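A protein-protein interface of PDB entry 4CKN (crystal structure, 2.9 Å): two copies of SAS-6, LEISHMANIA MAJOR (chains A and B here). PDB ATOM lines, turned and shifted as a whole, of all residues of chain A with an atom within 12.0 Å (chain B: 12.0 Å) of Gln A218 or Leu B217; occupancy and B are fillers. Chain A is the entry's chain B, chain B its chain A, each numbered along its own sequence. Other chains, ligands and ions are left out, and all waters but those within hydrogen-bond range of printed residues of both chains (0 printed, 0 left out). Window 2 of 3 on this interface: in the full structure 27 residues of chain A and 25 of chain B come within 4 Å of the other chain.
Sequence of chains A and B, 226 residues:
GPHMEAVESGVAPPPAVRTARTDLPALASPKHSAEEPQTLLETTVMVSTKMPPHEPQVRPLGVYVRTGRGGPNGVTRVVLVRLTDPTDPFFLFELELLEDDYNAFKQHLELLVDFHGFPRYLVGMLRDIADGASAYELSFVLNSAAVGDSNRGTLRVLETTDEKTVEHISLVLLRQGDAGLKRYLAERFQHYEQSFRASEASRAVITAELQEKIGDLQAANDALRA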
ATOM      1  N   GLU A 209      33.385  12.674 -10.917  1.00  0.00           N
ATOM      2  CA  GLU A 209      32.785  13.345 -12.085  1.00  0.00           C
ATOM      3  C   GLU A 209      31.255  13.437 -11.995  1.00  0.00           C
ATOM      4  O   GLU A 209      30.669  14.467 -12.348  1.00  0.00           O
ATOM      5  CB  GLU A 209      33.190  12.643 -13.402  1.00  0.00           C
ATOM      6  CG  GLU A 209      33.965  13.511 -14.384  1.00  0.00           C
ATOM      7  CD  GLU A 209      34.714  12.708 -15.436  1.00  0.00           C
ATOM      8  OE1 GLU A 209      34.427  11.495 -15.609  1.00  0.00           O
ATOM      9  OE2 GLU A 209      35.589  13.308 -16.097  1.00  0.00           O
ATOM     10  N   LEU A 210      30.622  12.367 -11.515  1.00  0.00           N
ATOM     11  CA  LEU A 210      29.164  12.324 -11.366  1.00  0.00           C
ATOM     12  C   LEU A 210      28.702  12.946 -10.052  1.00  0.00           C
ATOM     13  O   LEU A 210      27.659  13.590 -10.015  1.00  0.00           O
ATOM     14  CB  LEU A 210      28.632  10.890 -11.477  1.00  0.00           C
ATOM     15  CG  LEU A 210      28.838  10.131 -12.796  1.00  0.00           C
ATOM     16  CD1 LEU A 210      27.953   8.894 -12.826  1.00  0.00           C
ATOM     17  CD2 LEU A 210      28.566  10.989 -14.024  1.00  0.00           C
ATOM     18  N   GLN A 211      29.471  12.764  -8.980  1.00  0.00           N
ATOM     19  CA  GLN A 211      29.160  13.418  -7.701  1.00  0.00           C
ATOM     20  C   GLN A 211      29.157  14.956  -7.805  1.00  0.00           C
ATOM     21  O   GLN A 211      28.381  15.630  -7.108  1.00  0.00           O
ATOM     22  CB  GLN A 211      30.146  12.971  -6.625  1.00  0.00           C
ATOM     23  CG  GLN A 211      29.757  13.371  -5.207  1.00  0.00           C
ATOM     24  CD  GLN A 211      28.461  12.729  -4.694  1.00  0.00           C
ATOM     25  OE1 GLN A 211      27.761  11.992  -5.406  1.00  0.00           O
ATOM     26  NE2 GLN A 211      28.136  13.019  -3.443  1.00  0.00           N
ATOM     27  N   GLU A 212      30.029  15.485  -8.669  1.00  0.00           N
ATOM     28  CA  GLU A 212      30.066  16.919  -9.009  1.00  0.00           C
ATOM     29  C   GLU A 212      28.827  17.295  -9.841  1.00  0.00           C
ATOM     30  O   GLU A 212      28.240  18.369  -9.654  1.00  0.00           O
ATOM     31  CB  GLU A 212      31.416  17.289  -9.736  1.00  0.00           C
ATOM     32  CG  GLU A 212      32.515  17.745  -8.768  1.00  0.00           C
ATOM     33  CD  GLU A 212      33.922  17.759  -9.365  1.00  0.00           C
ATOM     34  OE1 GLU A 212      34.541  16.683  -9.550  1.00  0.00           O
ATOM     35  OE2 GLU A 212      34.436  18.875  -9.615  1.00  0.00           O
ATOM     36  N   LYS A 213      28.403  16.388 -10.724  1.00  0.00           N
ATOM     37  CA  LYS A 213      27.168  16.560 -11.503  1.00  0.00           C
ATOM     38  C   LYS A 213      25.874  16.353 -10.676  1.00  0.00           C
ATOM     39  O   LYS A 213      24.813  16.836 -11.060  1.00  0.00           O
ATOM     40  CB  LYS A 213      27.172  15.669 -12.764  1.00  0.00           C
ATOM     41  CG  LYS A 213      27.805  16.329 -13.978  1.00  0.00           C
ATOM     42  CD  LYS A 213      27.632  15.471 -15.215  1.00  0.00           C
ATOM     43  CE  LYS A 213      28.263  16.066 -16.426  1.00  0.00           C
ATOM     44  NZ  LYS A 213      29.571  16.718 -16.178  1.00  0.00           N
ATOM     45  N   ILE A 214      25.969  15.638  -9.553  1.00  0.00           N
ATOM     46  CA  ILE A 214      24.896  15.585  -8.548  1.00  0.00           C
ATOM     47  C   ILE A 214      24.962  16.843  -7.683  1.00  0.00           C
ATOM     48  O   ILE A 214      23.929  17.411  -7.318  1.00  0.00           O
ATOM     49  CB  ILE A 214      25.017  14.334  -7.635  1.00  0.00           C
ATOM     50  CG1 ILE A 214      24.817  13.042  -8.441  1.00  0.00           C
ATOM     51  CG2 ILE A 214      24.030  14.388  -6.470  1.00  0.00           C
ATOM     52  CD1 ILE A 214      23.451  12.872  -9.071  1.00  0.00           C
ATOM     53  N   GLY A 215      26.186  17.262  -7.361  1.00  0.00           N
ATOM     54  CA  GLY A 215      26.421  18.448  -6.543  1.00  0.00           C
ATOM     55  C   GLY A 215      26.072  19.779  -7.200  1.00  0.00           C
ATOM     56  O   GLY A 215      25.908  20.778  -6.498  1.00  0.00           O
ATOM     57  N   ASP A 216      25.970  19.801  -8.534  1.00  0.00           N
ATOM     58  CA  ASP A 216      25.613  21.017  -9.286  1.00  0.00           C
ATOM     59  C   ASP A 216      24.131  21.073  -9.685  1.00  0.00           C
ATOM     60  O   ASP A 216      23.545  22.152  -9.691  1.00  0.00           O
ATOM     61  CB  ASP A 216      26.462  21.156 -10.563  1.00  0.00           C
ATOM     62  CG  ASP A 216      27.926  21.498 -10.281  1.00  0.00           C
ATOM     63  OD1 ASP A 216      28.225  22.108  -9.234  1.00  0.00           O
ATOM     64  OD2 ASP A 216      28.782  21.186 -11.138  1.00  0.00           O
ATOM     65  N   LEU A 217      23.534  19.930 -10.027  1.00  0.00           N
ATOM     66  CA  LEU A 217      22.139  19.894 -10.499  1.00  0.00           C
ATOM     67  C   LEU A 217      21.137  20.156  -9.375  1.00  0.00           C
ATOM     68  O   LEU A 217      20.065  20.709  -9.629  1.00  0.00           O
ATOM     69  CB  LEU A 217      21.816  18.561 -11.199  1.00  0.00           C
ATOM     70  CG  LEU A 217      22.454  18.321 -12.576  1.00  0.00           C
ATOM     71  CD1 LEU A 217      21.939  17.023 -13.178  1.00  0.00           C
ATOM     72  CD2 LEU A 217      22.226  19.475 -13.545  1.00  0.00           C
ATOM     73  N   GLN A 218      21.487  19.780  -8.143  1.00  0.00           N
ATOM     74  CA  GLN A 218      20.609  20.005  -6.987  1.00  0.00           C
ATOM     75  C   GLN A 218      20.490  21.488  -6.594  1.00  0.00           C
ATOM     76  O   GLN A 218      19.399  21.955  -6.253  1.00  0.00           O
ATOM     77  CB  GLN A 218      21.052  19.162  -5.780  1.00  0.00           C
ATOM     78  CG  GLN A 218      20.739  17.682  -5.920  1.00  0.00           C
ATOM     79  CD  GLN A 218      20.979  16.894  -4.641  1.00  0.00           C
ATOM     80  OE1 GLN A 218      21.645  17.363  -3.717  1.00  0.00           O
ATOM     81  NE2 GLN A 218      20.428  15.690  -4.581  1.00  0.00           N
ATOM     82  N   ALA A 219      21.603  22.220  -6.633  1.00  0.00           N
ATOM     83  CA  ALA A 219      21.592  23.654  -6.305  1.00  0.00           C
ATOM     84  C   ALA A 219      20.879  24.489  -7.382  1.00  0.00           C
ATOM     85  O   ALA A 219      20.163  25.435  -7.047  1.00  0.00           O
ATOM     86  CB  ALA A 219      23.009  24.169  -6.083  1.00  0.00           C
ATOM     87  N   ALA A 220      21.081  24.134  -8.658  1.00  0.00           N
ATOM     88  CA  ALA A 220      20.442  24.801  -9.805  1.00  0.00           C
ATOM     89  C   ALA A 220      18.981  24.366  -9.924  1.00  0.00           C
ATOM     90  O   ALA A 220      18.132  25.147 -10.343  1.00  0.00           O
ATOM     91  CB  ALA A 220      21.192  24.492 -11.103  1.00  0.00           C
ATOM     92  N   ALA B 208      25.423   3.234 -12.020  1.00  0.00           N
ATOM     93  CA  ALA B 208      23.961   3.137 -12.089  1.00  0.00           C
ATOM     94  C   ALA B 208      23.265   3.906 -10.961  1.00  0.00           C
ATOM     95  O   ALA B 208      22.289   4.619 -11.198  1.00  0.00           O
ATOM     96  CB  ALA B 208      23.534   1.678 -12.072  1.00  0.00           C
ATOM     97  N   GLU B 209      23.766   3.760  -9.738  1.00  0.00           N
ATOM     98  CA  GLU B 209      23.207   4.468  -8.584  1.00  0.00           C
ATOM     99  C   GLU B 209      23.200   5.986  -8.753  1.00  0.00           C
ATOM    100  O   GLU B 209      22.255   6.649  -8.337  1.00  0.00           O
ATOM    101  CB  GLU B 209      23.981   4.151  -7.312  1.00  0.00           C
ATOM    102  CG  GLU B 209      23.133   4.416  -6.047  1.00  0.00           C
ATOM    103  CD  GLU B 209      22.486   3.182  -5.458  1.00  0.00           C
ATOM    104  OE1 GLU B 209      22.959   2.056  -5.717  1.00  0.00           O
ATOM    105  OE2 GLU B 209      21.507   3.345  -4.703  1.00  0.00           O
ATOM    106  N   LEU B 210      24.276   6.526  -9.322  1.00  0.00           N
ATOM    107  CA  LEU B 210      24.398   7.969  -9.560  1.00  0.00           C
ATOM    108  C   LEU B 210      23.729   8.384 -10.879  1.00  0.00           C
ATOM    109  O   LEU B 210      23.153   9.459 -10.954  1.00  0.00           O
ATOM    110  CB  LEU B 210      25.870   8.409  -9.548  1.00  0.00           C
ATOM    111  CG  LEU B 210      26.695   8.215  -8.263  1.00  0.00           C
ATOM    112  CD1 LEU B 210      27.990   9.007  -8.353  1.00  0.00           C
ATOM    113  CD2 LEU B 210      25.933   8.610  -7.007  1.00  0.00           C
ATOM    114  N   GLN B 211      23.799   7.529 -11.902  1.00  0.00           N
ATOM    115  CA  GLN B 211      23.090   7.756 -13.181  1.00  0.00           C
ATOM    116  C   GLN B 211      21.564   7.889 -12.967  1.00  0.00           C
ATOM    117  O   GLN B 211      20.880   8.655 -13.666  1.00  0.00           O
ATOM    118  CB  GLN B 211      23.403   6.647 -14.233  1.00  0.00           C
ATOM    119  CG  GLN B 211      24.573   6.955 -15.184  1.00  0.00           C
ATOM    120  CD  GLN B 211      24.422   8.293 -15.879  1.00  0.00           C
ATOM    121  OE1 GLN B 211      25.228   9.200 -15.680  1.00  0.00           O
ATOM    122  NE2 GLN B 211      23.373   8.432 -16.672  1.00  0.00           N
ATOM    123  N   GLU B 212      21.040   7.144 -11.994  1.00  0.00           N
ATOM    124  CA  GLU B 212      19.638   7.273 -11.597  1.00  0.00           C
ATOM    125  C   GLU B 212      19.395   8.579 -10.842  1.00  0.00           C
ATOM    126  O   GLU B 212      18.332   9.173 -10.973  1.00  0.00           O
ATOM    127  CB  GLU B 212      19.197   6.090 -10.740  1.00  0.00           C
ATOM    128  CG  GLU B 212      17.723   5.705 -10.877  1.00  0.00           C
ATOM    129  CD  GLU B 212      17.367   4.456 -10.086  1.00  0.00           C
ATOM    130  OE1 GLU B 212      17.926   4.278  -8.982  1.00  0.00           O
ATOM    131  OE2 GLU B 212      16.540   3.646 -10.580  1.00  0.00           O
ATOM    132  N   LYS B 213      20.367   9.007 -10.039  1.00  0.00           N
ATOM    133  CA  LYS B 213      20.300  10.312  -9.362  1.00  0.00           C
ATOM    134  C   LYS B 213      20.543  11.496 -10.326  1.00  0.00           C
ATOM    135  O   LYS B 213      20.154  12.619 -10.027  1.00  0.00           O
ATOM    136  CB  LYS B 213      21.238  10.344  -8.154  1.00  0.00           C
ATOM    137  CG  LYS B 213      20.838  11.256  -6.993  1.00  0.00           C
ATOM    138  CD  LYS B 213      21.915  11.301  -5.902  1.00  0.00           C
ATOM    139  CE  LYS B 213      21.511  12.220  -4.703  1.00  0.00           C
ATOM    140  NZ  LYS B 213      21.983  11.756  -3.358  1.00  0.00           N
ATOM    141  N   ILE B 214      21.179  11.242 -11.471  1.00  0.00           N
ATOM    142  CA  ILE B 214      21.242  12.212 -12.578  1.00  0.00           C
ATOM    143  C   ILE B 214      19.935  12.146 -13.366  1.00  0.00           C
ATOM    144  O   ILE B 214      19.415  13.170 -13.803  1.00  0.00           O
ATOM    145  CB  ILE B 214      22.431  11.924 -13.534  1.00  0.00           C
ATOM    146  CG1 ILE B 214      23.780  12.108 -12.817  1.00  0.00           C
ATOM    147  CG2 ILE B 214      22.369  12.799 -14.786  1.00  0.00           C
ATOM    148  CD1 ILE B 214      24.076  13.515 -12.335  1.00  0.00           C
ATOM    149  N   GLY B 215      19.413  10.934 -13.534  1.00  0.00           N
ATOM    150  CA  GLY B 215      18.162  10.706 -14.257  1.00  0.00           C
ATOM    151  C   GLY B 215      16.898  11.184 -13.553  1.00  0.00           C
ATOM    152  O   GLY B 215      15.868  11.344 -14.200  1.00  0.00           O
ATOM    153  N   ASP B 216      16.967  11.397 -12.235  1.00  0.00           N
ATOM    154  CA  ASP B 216      15.822  11.910 -11.453  1.00  0.00           C
ATOM    155  C   ASP B 216      15.898  13.432 -11.272  1.00  0.00           C
ATOM    156  O   ASP B 216      14.873  14.097 -11.208  1.00  0.00           O
ATOM    157  CB  ASP B 216      15.729  11.231 -10.073  1.00  0.00           C
ATOM    158  CG  ASP B 216      15.278   9.774 -10.153  1.00  0.00           C
ATOM    159  OD1 ASP B 216      14.584   9.402 -11.128  1.00  0.00           O
ATOM    160  OD2 ASP B 216      15.603   8.999  -9.226  1.00  0.00           O
ATOM    161  N   LEU B 217      17.110  13.972 -11.172  1.00  0.00           N
ATOM    162  CA  LEU B 217      17.329  15.423 -11.156  1.00  0.00           C
ATOM    163  C   LEU B 217      17.006  16.032 -12.530  1.00  0.00           C
ATOM    164  O   LEU B 217      16.570  17.173 -12.598  1.00  0.00           O
ATOM    165  CB  LEU B 217      18.768  15.744 -10.710  1.00  0.00           C
ATOM    166  CG  LEU B 217      19.104  15.477  -9.231  1.00  0.00           C
ATOM    167  CD1 LEU B 217      20.527  15.924  -8.928  1.00  0.00           C
ATOM    168  CD2 LEU B 217      18.134  16.158  -8.272  1.00  0.00           C
ATOM    169  N   GLN B 218      17.178  15.262 -13.607  1.00  0.00           N
ATOM    170  CA  GLN B 218      16.822  15.714 -14.960  1.00  0.00           C
ATOM    171  C   GLN B 218      15.313  15.841 -15.183  1.00  0.00           C
ATOM    172  O   GLN B 218      14.854  16.790 -15.823  1.00  0.00           O
ATOM    173  CB  GLN B 218      17.366  14.726 -16.001  1.00  0.00           C
ATOM    174  CG  GLN B 218      17.254  15.186 -17.471  1.00  0.00           C
ATOM    175  CD  GLN B 218      18.199  16.328 -17.824  1.00  0.00           C
ATOM    176  OE1 GLN B 218      18.787  16.954 -16.947  1.00  0.00           O
ATOM    177  NE2 GLN B 218      18.352  16.598 -19.120  1.00  0.00           N
ATOM    178  N   ALA B 219      14.552  14.859 -14.699  1.00  0.00           N
ATOM    179  CA  ALA B 219      13.093  14.858 -14.869  1.00  0.00           C
ATOM    180  C   ALA B 219      12.414  15.955 -14.033  1.00  0.00           C
ATOM    181  O   ALA B 219      11.451  16.574 -14.496  1.00  0.00           O
ATOM    182  CB  ALA B 219      12.511  13.491 -14.534  1.00  0.00           C
ATOM    183  N   ALA B 220      12.931  16.191 -12.822  1.00  0.00           N
ATOM    184  CA  ALA B 220      12.458  17.265 -11.937  1.00  0.00           C
ATOM    185  C   ALA B 220      12.960  18.617 -12.441  1.00  0.00           C
ATOM    186  O   ALA B 220      12.289  19.634 -12.278  1.00  0.00           O
ATOM    187  CB  ALA B 220      12.918  17.029 -10.494  1.00  0.00           C
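Leu A210 touches Gln B211, but with the chains exchanged Gln A211 does not touch Leu B210 (4.1 Å).
Lys A213 touches Ile B214, and with the chains exchanged Ile A214 touches Lys B213.
Ile A214 touches Leu B210, but with the chains exchanged Leu A210 does not touch Ile B214 (4.3 Å).
Leu B217 touches its own counterpart, Leu A217.
Positions printed for both chains: 209, 210, 211, 212, 213, 214, 215, 216, 217, 218, 219 and 220.
Of the 9 pairs that touch across the chains among the printed residues, 5 have their exchanged pair printed and touching as well.
Among the printed residues, merely in contact across the chains: Leu A210 with Leu B210, Leu A210 with Gln B211, Lys A213 with Ile B214, Ile A214 with Leu B210, Ile A214 with Lys B213, Ile A214 with Ile B214, Leu A217 with Leu B217, Gln A218 with Lys B213 and Gln A218 with Leu B217.
Of chain B, only Lys B213 and Leu B217 come within 4 Å of Gln A218.
Of chain A, only Leu A217 and Gln A218 come within 4 Å of Leu B217.
Of chain B, only Leu B210 (3.9 Å), Lys B213 (3.4 Å) and Ile B214 (3.4 Å) come within 4 Å of Ile A214.
Leu A217 touches one residue of chain B.
No residue of chain B comes within 4 Å of Ala A220.
Of chain A, only Ile A214 (3.4 Å) and Gln A218 (3.6 Å) come within 4 Å of Lys B213.
Of chain A, only Lys A213 and Ile A214 come within 4 Å of Ile B214.
No residue of chain A comes within 4 Å of Gly B215.
No residue of chain A comes within 4 Å of Asp B216.
No residue of chain A comes within 4 Å of Gln B218.
No residue of chain A comes within 4 Å of Ala B219.
No residue of chain A comes within 4 Å of Ala B220.
Of the printed residues of chain A, Gln B211 touches Leu A210 (3.96 Å).
Of the printed residues of chain B, Lys A213 touches Ile B214.
Of the printed residues of chain B, Leu A210 touches Leu B210 (3.7 Å) and Gln B211 (3.96 Å).
Asp A216 touches none of the printed residues of chain B.
Ala B208 touches none of the printed residues of chain A.
The nearest residue of chain B that does not touch Gln A218 is Ile B214 (8.0 Å).
The nearest printed residue of chain A that does not touch Gln B211 is Ile A214 (6.1 Å).
Hydrophobic or aromatic side chains of chain A within 4 Å of the printed part of chain B: Leu A210, Ile A214 and Leu A217.
Hydrophobic or aromatic side chains of chain B within 4 Å of the printed part of chain A: Leu B210, Ile B214 and Leu B217.
Among the printed residues, no Asp or Glu carboxylate lies within 4 Å of a Lys or Arg side-chain nitrogen of the other chain.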
